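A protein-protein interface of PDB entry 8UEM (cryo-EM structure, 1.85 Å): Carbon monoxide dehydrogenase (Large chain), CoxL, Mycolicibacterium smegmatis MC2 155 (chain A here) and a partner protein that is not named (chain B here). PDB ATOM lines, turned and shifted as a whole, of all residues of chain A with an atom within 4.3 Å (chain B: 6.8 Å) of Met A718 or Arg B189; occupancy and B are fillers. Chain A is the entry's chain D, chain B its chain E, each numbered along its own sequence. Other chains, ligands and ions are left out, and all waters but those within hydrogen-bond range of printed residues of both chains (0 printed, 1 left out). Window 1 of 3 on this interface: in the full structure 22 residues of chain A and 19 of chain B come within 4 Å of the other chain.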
ATOM      1  N   SER A 716      14.040 -22.482  -4.809  1.00  0.00           N
ATOM      2  CA  SER A 716      14.010 -23.846  -4.314  1.00  0.00           C
ATOM      3  C   SER A 716      15.431 -24.289  -4.019  1.00  0.00           C
ATOM      4  O   SER A 716      16.400 -23.660  -4.450  1.00  0.00           O
ATOM      5  CB  SER A 716      13.344 -24.795  -5.316  1.00  0.00           C
ATOM      6  OG  SER A 716      14.264 -25.229  -6.301  1.00  0.00           O
ATOM      7  N   LEU A 717      15.538 -25.379  -3.267  1.00  0.00           N
ATOM      8  CA  LEU A 717      16.832 -25.976  -2.998  1.00  0.00           C
ATOM      9  C   LEU A 717      17.427 -26.650  -4.223  1.00  0.00           C
ATOM     10  O   LEU A 717      18.595 -27.043  -4.183  1.00  0.00           O
ATOM     11  CB  LEU A 717      16.705 -26.959  -1.842  1.00  0.00           C
ATOM     12  CG  LEU A 717      16.434 -26.217  -0.536  1.00  0.00           C
ATOM     13  CD1 LEU A 717      16.660 -27.104   0.673  1.00  0.00           C
ATOM     14  CD2 LEU A 717      17.304 -24.960  -0.458  1.00  0.00           C
ATOM     15  N   MET A 718      16.655 -26.805  -5.299  1.00  0.00           N
ATOM     16  CA  MET A 718      17.257 -27.178  -6.572  1.00  0.00           C
ATOM     17  C   MET A 718      18.057 -26.022  -7.152  1.00  0.00           C
ATOM     18  O   MET A 718      19.120 -26.229  -7.744  1.00  0.00           O
ATOM     19  CB  MET A 718      16.183 -27.617  -7.563  1.00  0.00           C
ATOM     20  CG  MET A 718      15.207 -28.631  -7.026  1.00  0.00           C
ATOM     21  SD  MET A 718      14.330 -29.488  -8.345  1.00  0.00           S
ATOM     22  CE  MET A 718      14.748 -28.469  -9.750  1.00  0.00           C
ATOM     23  N   ASP A 719      17.559 -24.797  -6.993  1.00  0.00           N
ATOM     24  CA  ASP A 719      18.182 -23.620  -7.582  1.00  0.00           C
ATOM     25  C   ASP A 719      19.047 -22.836  -6.612  1.00  0.00           C
ATOM     26  O   ASP A 719      20.004 -22.187  -7.042  1.00  0.00           O
ATOM     27  CB  ASP A 719      17.113 -22.692  -8.155  1.00  0.00           C
ATOM     28  CG  ASP A 719      16.143 -23.417  -9.049  1.00  0.00           C
ATOM     29  OD1 ASP A 719      16.602 -24.067 -10.011  1.00  0.00           O
ATOM     30  OD2 ASP A 719      14.926 -23.339  -8.791  1.00  0.00           O
ATOM     31  N   TYR A 720      18.736 -22.867  -5.326  1.00  0.00           N
ATOM     32  CA  TYR A 720      19.594 -22.281  -4.305  1.00  0.00           C
ATOM     33  C   TYR A 720      20.401 -23.416  -3.693  1.00  0.00           C
ATOM     34  O   TYR A 720      19.889 -24.189  -2.883  1.00  0.00           O
ATOM     35  CB  TYR A 720      18.789 -21.539  -3.249  1.00  0.00           C
ATOM     36  CG  TYR A 720      19.682 -20.814  -2.278  1.00  0.00           C
ATOM     37  CD1 TYR A 720      20.360 -19.664  -2.662  1.00  0.00           C
ATOM     38  CD2 TYR A 720      19.865 -21.286  -0.990  1.00  0.00           C
ATOM     39  CE1 TYR A 720      21.174 -19.001  -1.788  1.00  0.00           C
ATOM     40  CE2 TYR A 720      20.679 -20.626  -0.108  1.00  0.00           C
ATOM     41  CZ  TYR A 720      21.339 -19.488  -0.512  1.00  0.00           C
ATOM     42  OH  TYR A 720      22.157 -18.828   0.368  1.00  0.00           O
ATOM     43  N   LEU A 721      21.671 -23.495  -4.069  1.00  0.00           N
ATOM     44  CA  LEU A 721      22.503 -24.653  -3.772  1.00  0.00           C
ATOM     45  C   LEU A 721      23.238 -24.415  -2.463  1.00  0.00           C
ATOM     46  O   LEU A 721      24.084 -23.522  -2.372  1.00  0.00           O
ATOM     47  CB  LEU A 721      23.478 -24.918  -4.915  1.00  0.00           C
ATOM     48  CG  LEU A 721      22.821 -25.204  -6.266  1.00  0.00           C
ATOM     49  CD1 LEU A 721      23.849 -25.632  -7.285  1.00  0.00           C
ATOM     50  CD2 LEU A 721      21.724 -26.244  -6.120  1.00  0.00           C
ATOM     51  N   PRO A 784      31.308 -23.178 -11.337  1.00  0.00           N
ATOM     52  CA  PRO A 784      32.226 -23.620 -12.396  1.00  0.00           C
ATOM     53  C   PRO A 784      32.191 -22.722 -13.616  1.00  0.00           C
ATOM     54  O   PRO A 784      33.245 -22.384 -14.167  1.00  0.00           O
ATOM     55  CB  PRO A 784      31.729 -25.038 -12.708  1.00  0.00           C
ATOM     56  CG  PRO A 784      31.065 -25.484 -11.448  1.00  0.00           C
ATOM     57  CD  PRO A 784      30.434 -24.264 -10.865  1.00  0.00           C
ATOM     58  N   PRO B  40       7.888 -34.867  -6.987  1.00  0.00           N
ATOM     59  CA  PRO B  40       8.218 -33.434  -6.940  1.00  0.00           C
ATOM     60  C   PRO B  40       7.397 -32.601  -7.910  1.00  0.00           C
ATOM     61  O   PRO B  40       6.987 -31.488  -7.562  1.00  0.00           O
ATOM     62  CB  PRO B  40       9.714 -33.408  -7.279  1.00  0.00           C
ATOM     63  CG  PRO B  40      10.211 -34.741  -6.850  1.00  0.00           C
ATOM     64  CD  PRO B  40       9.090 -35.706  -7.126  1.00  0.00           C
ATOM     65  N   LEU B  44       4.810 -29.674  -6.725  1.00  0.00           N
ATOM     66  CA  LEU B  44       4.813 -28.350  -7.326  1.00  0.00           C
ATOM     67  C   LEU B  44       3.592 -28.111  -8.194  1.00  0.00           C
ATOM     68  O   LEU B  44       3.419 -27.004  -8.708  1.00  0.00           O
ATOM     69  CB  LEU B  44       6.083 -28.145  -8.150  1.00  0.00           C
ATOM     70  CG  LEU B  44       7.384 -28.465  -7.415  1.00  0.00           C
ATOM     71  CD1 LEU B  44       8.585 -28.221  -8.300  1.00  0.00           C
ATOM     72  CD2 LEU B  44       7.477 -27.652  -6.134  1.00  0.00           C
ATOM     73  N   VAL B 187      29.490 -32.171 -14.848  1.00  0.00           N
ATOM     74  CA  VAL B 187      29.801 -30.972 -14.095  1.00  0.00           C
ATOM     75  C   VAL B 187      28.493 -30.425 -13.560  1.00  0.00           C
ATOM     76  O   VAL B 187      27.575 -30.095 -14.330  1.00  0.00           O
ATOM     77  CB  VAL B 187      30.540 -29.921 -14.931  1.00  0.00           C
ATOM     78  CG1 VAL B 187      30.489 -28.582 -14.218  1.00  0.00           C
ATOM     79  CG2 VAL B 187      31.975 -30.346 -15.147  1.00  0.00           C
ATOM     80  N   GLU B 188      28.437 -30.331 -12.239  1.00  0.00           N
ATOM     81  CA  GLU B 188      27.329 -29.795 -11.477  1.00  0.00           C
ATOM     82  C   GLU B 188      27.875 -28.735 -10.532  1.00  0.00           C
ATOM     83  O   GLU B 188      29.026 -28.805 -10.102  1.00  0.00           O
ATOM     84  CB  GLU B 188      26.632 -30.908 -10.688  1.00  0.00           C
ATOM     85  CG  GLU B 188      27.514 -31.526  -9.614  1.00  0.00           C
ATOM     86  CD  GLU B 188      27.721 -33.014  -9.798  1.00  0.00           C
ATOM     87  OE1 GLU B 188      28.132 -33.434 -10.898  1.00  0.00           O
ATOM     88  OE2 GLU B 188      27.478 -33.765  -8.832  1.00  0.00           O
ATOM     89  N   ARG B 189      27.050 -27.737 -10.223  1.00  0.00           N
ATOM     90  CA  ARG B 189      27.475 -26.744  -9.244  1.00  0.00           C
ATOM     91  C   ARG B 189      27.666 -27.375  -7.874  1.00  0.00           C
ATOM     92  O   ARG B 189      28.553 -26.969  -7.118  1.00  0.00           O
ATOM     93  CB  ARG B 189      26.462 -25.607  -9.176  1.00  0.00           C
ATOM     94  CG  ARG B 189      26.399 -24.762 -10.429  1.00  0.00           C
ATOM     95  CD  ARG B 189      25.048 -24.112 -10.586  1.00  0.00           C
ATOM     96  NE  ARG B 189      23.966 -25.084 -10.508  1.00  0.00           N
ATOM     97  CZ  ARG B 189      22.702 -24.772 -10.271  1.00  0.00           C
ATOM     98  NH1 ARG B 189      22.327 -23.520 -10.078  1.00  0.00           N
ATOM     99  NH2 ARG B 189      21.791 -25.738 -10.236  1.00  0.00           N
ATOM    100  N   ARG B 190      26.860 -28.381  -7.552  1.00  0.00           N
ATOM    101  CA  ARG B 190      26.870 -29.007  -6.242  1.00  0.00           C
ATOM    102  C   ARG B 190      26.554 -30.485  -6.396  1.00  0.00           C
ATOM    103  O   ARG B 190      25.894 -30.903  -7.349  1.00  0.00           O
ATOM    104  CB  ARG B 190      25.859 -28.351  -5.297  1.00  0.00           C
ATOM    105  CG  ARG B 190      25.986 -28.810  -3.868  1.00  0.00           C
ATOM    106  CD  ARG B 190      24.826 -28.318  -3.036  1.00  0.00           C
ATOM    107  NE  ARG B 190      23.535 -28.731  -3.571  1.00  0.00           N
ATOM    108  CZ  ARG B 190      22.555 -29.249  -2.845  1.00  0.00           C
ATOM    109  NH1 ARG B 190      22.677 -29.425  -1.542  1.00  0.00           N
ATOM    110  NH2 ARG B 190      21.420 -29.597  -3.442  1.00  0.00           N
ATOM    111  N   VAL B 191      27.027 -31.272  -5.432  1.00  0.00           N
ATOM    112  CA  VAL B 191      26.695 -32.689  -5.407  1.00  0.00           C
ATOM    113  C   VAL B 191      25.186 -32.841  -5.314  1.00  0.00           C
ATOM    114  O   VAL B 191      24.526 -32.195  -4.493  1.00  0.00           O
ATOM    115  CB  VAL B 191      27.408 -33.385  -4.240  1.00  0.00           C
ATOM    116  CG1 VAL B 191      26.671 -34.646  -3.838  1.00  0.00           C
ATOM    117  CG2 VAL B 191      28.844 -33.691  -4.611  1.00  0.00           C
ATOM    118  N   ASP B 193      23.208 -31.809  -7.607  1.00  0.00           N
ATOM    119  CA  ASP B 193      22.664 -30.882  -8.581  1.00  0.00           C
ATOM    120  C   ASP B 193      22.645 -31.530  -9.958  1.00  0.00           C
ATOM    121  O   ASP B 193      23.476 -32.381 -10.284  1.00  0.00           O
ATOM    122  CB  ASP B 193      23.487 -29.593  -8.601  1.00  0.00           C
ATOM    123  CG  ASP B 193      22.968 -28.584  -9.601  1.00  0.00           C
ATOM    124  OD1 ASP B 193      21.737 -28.466  -9.740  1.00  0.00           O
ATOM    125  OD2 ASP B 193      23.795 -27.912 -10.249  1.00  0.00           O
ATOM    126  N   TRP B 194      21.664 -31.141 -10.761  1.00  0.00           N
ATOM    127  CA  TRP B 194      21.604 -31.626 -12.126  1.00  0.00           C
ATOM    128  C   TRP B 194      22.817 -31.131 -12.901  1.00  0.00           C
ATOM    129  O   TRP B 194      23.443 -30.130 -12.553  1.00  0.00           O
ATOM    130  CB  TRP B 194      20.318 -31.164 -12.797  1.00  0.00           C
ATOM    131  CG  TRP B 194      19.170 -32.070 -12.529  1.00  0.00           C
ATOM    132  CD1 TRP B 194      18.672 -33.028 -13.352  1.00  0.00           C
ATOM    133  CD2 TRP B 194      18.369 -32.097 -11.348  1.00  0.00           C
ATOM    134  NE1 TRP B 194      17.607 -33.654 -12.758  1.00  0.00           N
ATOM    135  CE2 TRP B 194      17.401 -33.101 -11.525  1.00  0.00           C
ATOM    136  CE3 TRP B 194      18.377 -31.373 -10.155  1.00  0.00           C
ATOM    137  CZ2 TRP B 194      16.448 -33.395 -10.560  1.00  0.00           C
ATOM    138  CZ3 TRP B 194      17.429 -31.668  -9.195  1.00  0.00           C
ATOM    139  CH2 TRP B 194      16.479 -32.674  -9.404  1.00  0.00           C
ATOM    140  N   ALA B 195      23.156 -31.862 -13.954  1.00  0.00           N
ATOM    141  CA  ALA B 195      24.368 -31.575 -14.701  1.00  0.00           C
ATOM    142  C   ALA B 195      24.365 -30.146 -15.211  1.00  0.00           C
ATOM    143  O   ALA B 195      23.456 -29.738 -15.940  1.00  0.00           O
ATOM    144  CB  ALA B 195      24.503 -32.549 -15.869  1.00  0.00           C
ATOM    145  N   VAL B 196      25.388 -29.380 -14.836  1.00  0.00           N
ATOM    146  CA  VAL B 196      25.702 -28.186 -15.609  1.00  0.00           C
ATOM    147  C   VAL B 196      25.920 -28.584 -17.053  1.00  0.00           C
ATOM    148  O   VAL B 196      25.369 -27.985 -17.983  1.00  0.00           O
ATOM    149  CB  VAL B 196      26.945 -27.480 -15.042  1.00  0.00           C
ATOM    150  CG1 VAL B 196      27.482 -26.487 -16.060  1.00  0.00           C
ATOM    151  CG2 VAL B 196      26.628 -26.825 -13.719  1.00  0.00           C
ATOM    152  N   THR B 261      21.117 -20.482 -15.071  1.00  0.00           N
ATOM    153  CA  THR B 261      21.699 -20.481 -13.734  1.00  0.00           C
ATOM    154  C   THR B 261      22.838 -21.482 -13.624  1.00  0.00           C
ATOM    155  O   THR B 261      23.736 -21.310 -12.795  1.00  0.00           O
ATOM    156  CB  THR B 261      20.630 -20.793 -12.687  1.00  0.00           C
ATOM    157  OG1 THR B 261      19.928 -21.985 -13.058  1.00  0.00           O
ATOM    158  CG2 THR B 261      19.644 -19.648 -12.577  1.00  0.00           C
ATOM    159  N   ARG B 262      22.819 -22.526 -14.442  1.00  0.00           N
ATOM    160  CA  ARG B 262      23.862 -23.537 -14.388  1.00  0.00           C
ATOM    161  C   ARG B 262      25.143 -23.102 -15.081  1.00  0.00           C
ATOM    162  O   ARG B 262      26.165 -23.775 -14.934  1.00  0.00           O
ATOM    163  CB  ARG B 262      23.353 -24.840 -15.000  1.00  0.00           C
ATOM    164  CG  ARG B 262      22.146 -25.406 -14.279  1.00  0.00           C
ATOM    165  CD  ARG B 262      22.139 -26.915 -14.317  1.00  0.00           C
ATOM    166  NE  ARG B 262      21.662 -27.502 -13.072  1.00  0.00           N
ATOM    167  CZ  ARG B 262      20.450 -27.316 -12.568  1.00  0.00           C
ATOM    168  NH1 ARG B 262      19.567 -26.530 -13.163  1.00  0.00           N
ATOM    169  NH2 ARG B 262      20.116 -27.932 -11.440  1.00  0.00           N
ATOM    170  N   GLY B 263      25.116 -22.006 -15.828  1.00  0.00           N
ATOM    171  CA  GLY B 263      26.321 -21.514 -16.455  1.00  0.00           C
ATOM    172  C   GLY B 263      26.098 -20.900 -17.818  1.00  0.00           C
ATOM    173  O   GLY B 263      25.020 -21.031 -18.400  1.00  0.00           O
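NH2 of Arg B189 is in salt-bridge range of OD1 of Asp B193.
N of Met A718 is in hydrogen-bond range of OG of Ser A716 (3.0 Å).
The side-chain carboxylate (OD1) of Asp B193 lies within salt-bridge range of the guanidinium group (NH2) of Arg B262 (2.4 Å).
NE of Arg B262 lies within hydrogen-bond range of O of Trp B194, 3.2 Å away.
Among the printed residues, merely in contact across the chains: Leu A721 with Arg B189, Met A718 with Arg B189, Leu A721 with Asp B193, Leu A717 with Arg B190, Met A718 with Trp B194, Leu A721 with Arg B190 and Met A718 with Asp B193.
Printed residues of chain B within 4 Å of Leu A717: Arg B190 (3.9 Å).
Of the printed residues of chain B, Leu A721 touches Arg B189 (3.2 Å), Arg B190 (3.9 Å) and Asp B193 (3.7 Å).
Printed residues of chain A within 4 Å of Arg B190: Leu A717 and Leu A721.
Printed residues of chain A within 4 Å of Asp B193: Met A718 (3.98 Å) and Leu A721 (3.7 Å).
The nearest residue of chain B that does not touch Met A718 is Arg B262 (4.2 Å).
The nearest residue of chain A that does not touch Arg B189 is Asp A719 (4.05 Å).
The nearest printed residue of chain A that does not touch Arg B190 is Tyr A720 (5.6 Å).
Of the 14 printed residues of chain B, 4 touch a printed residue of chain A.
Printed residues of chain B that touch a printed residue of chain A: Arg B189, Arg B190, Asp B193 and Trp B194.
Hydrophobic or aromatic side chains of chain B within 4 Å of the printed part of chain A: Trp B194.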
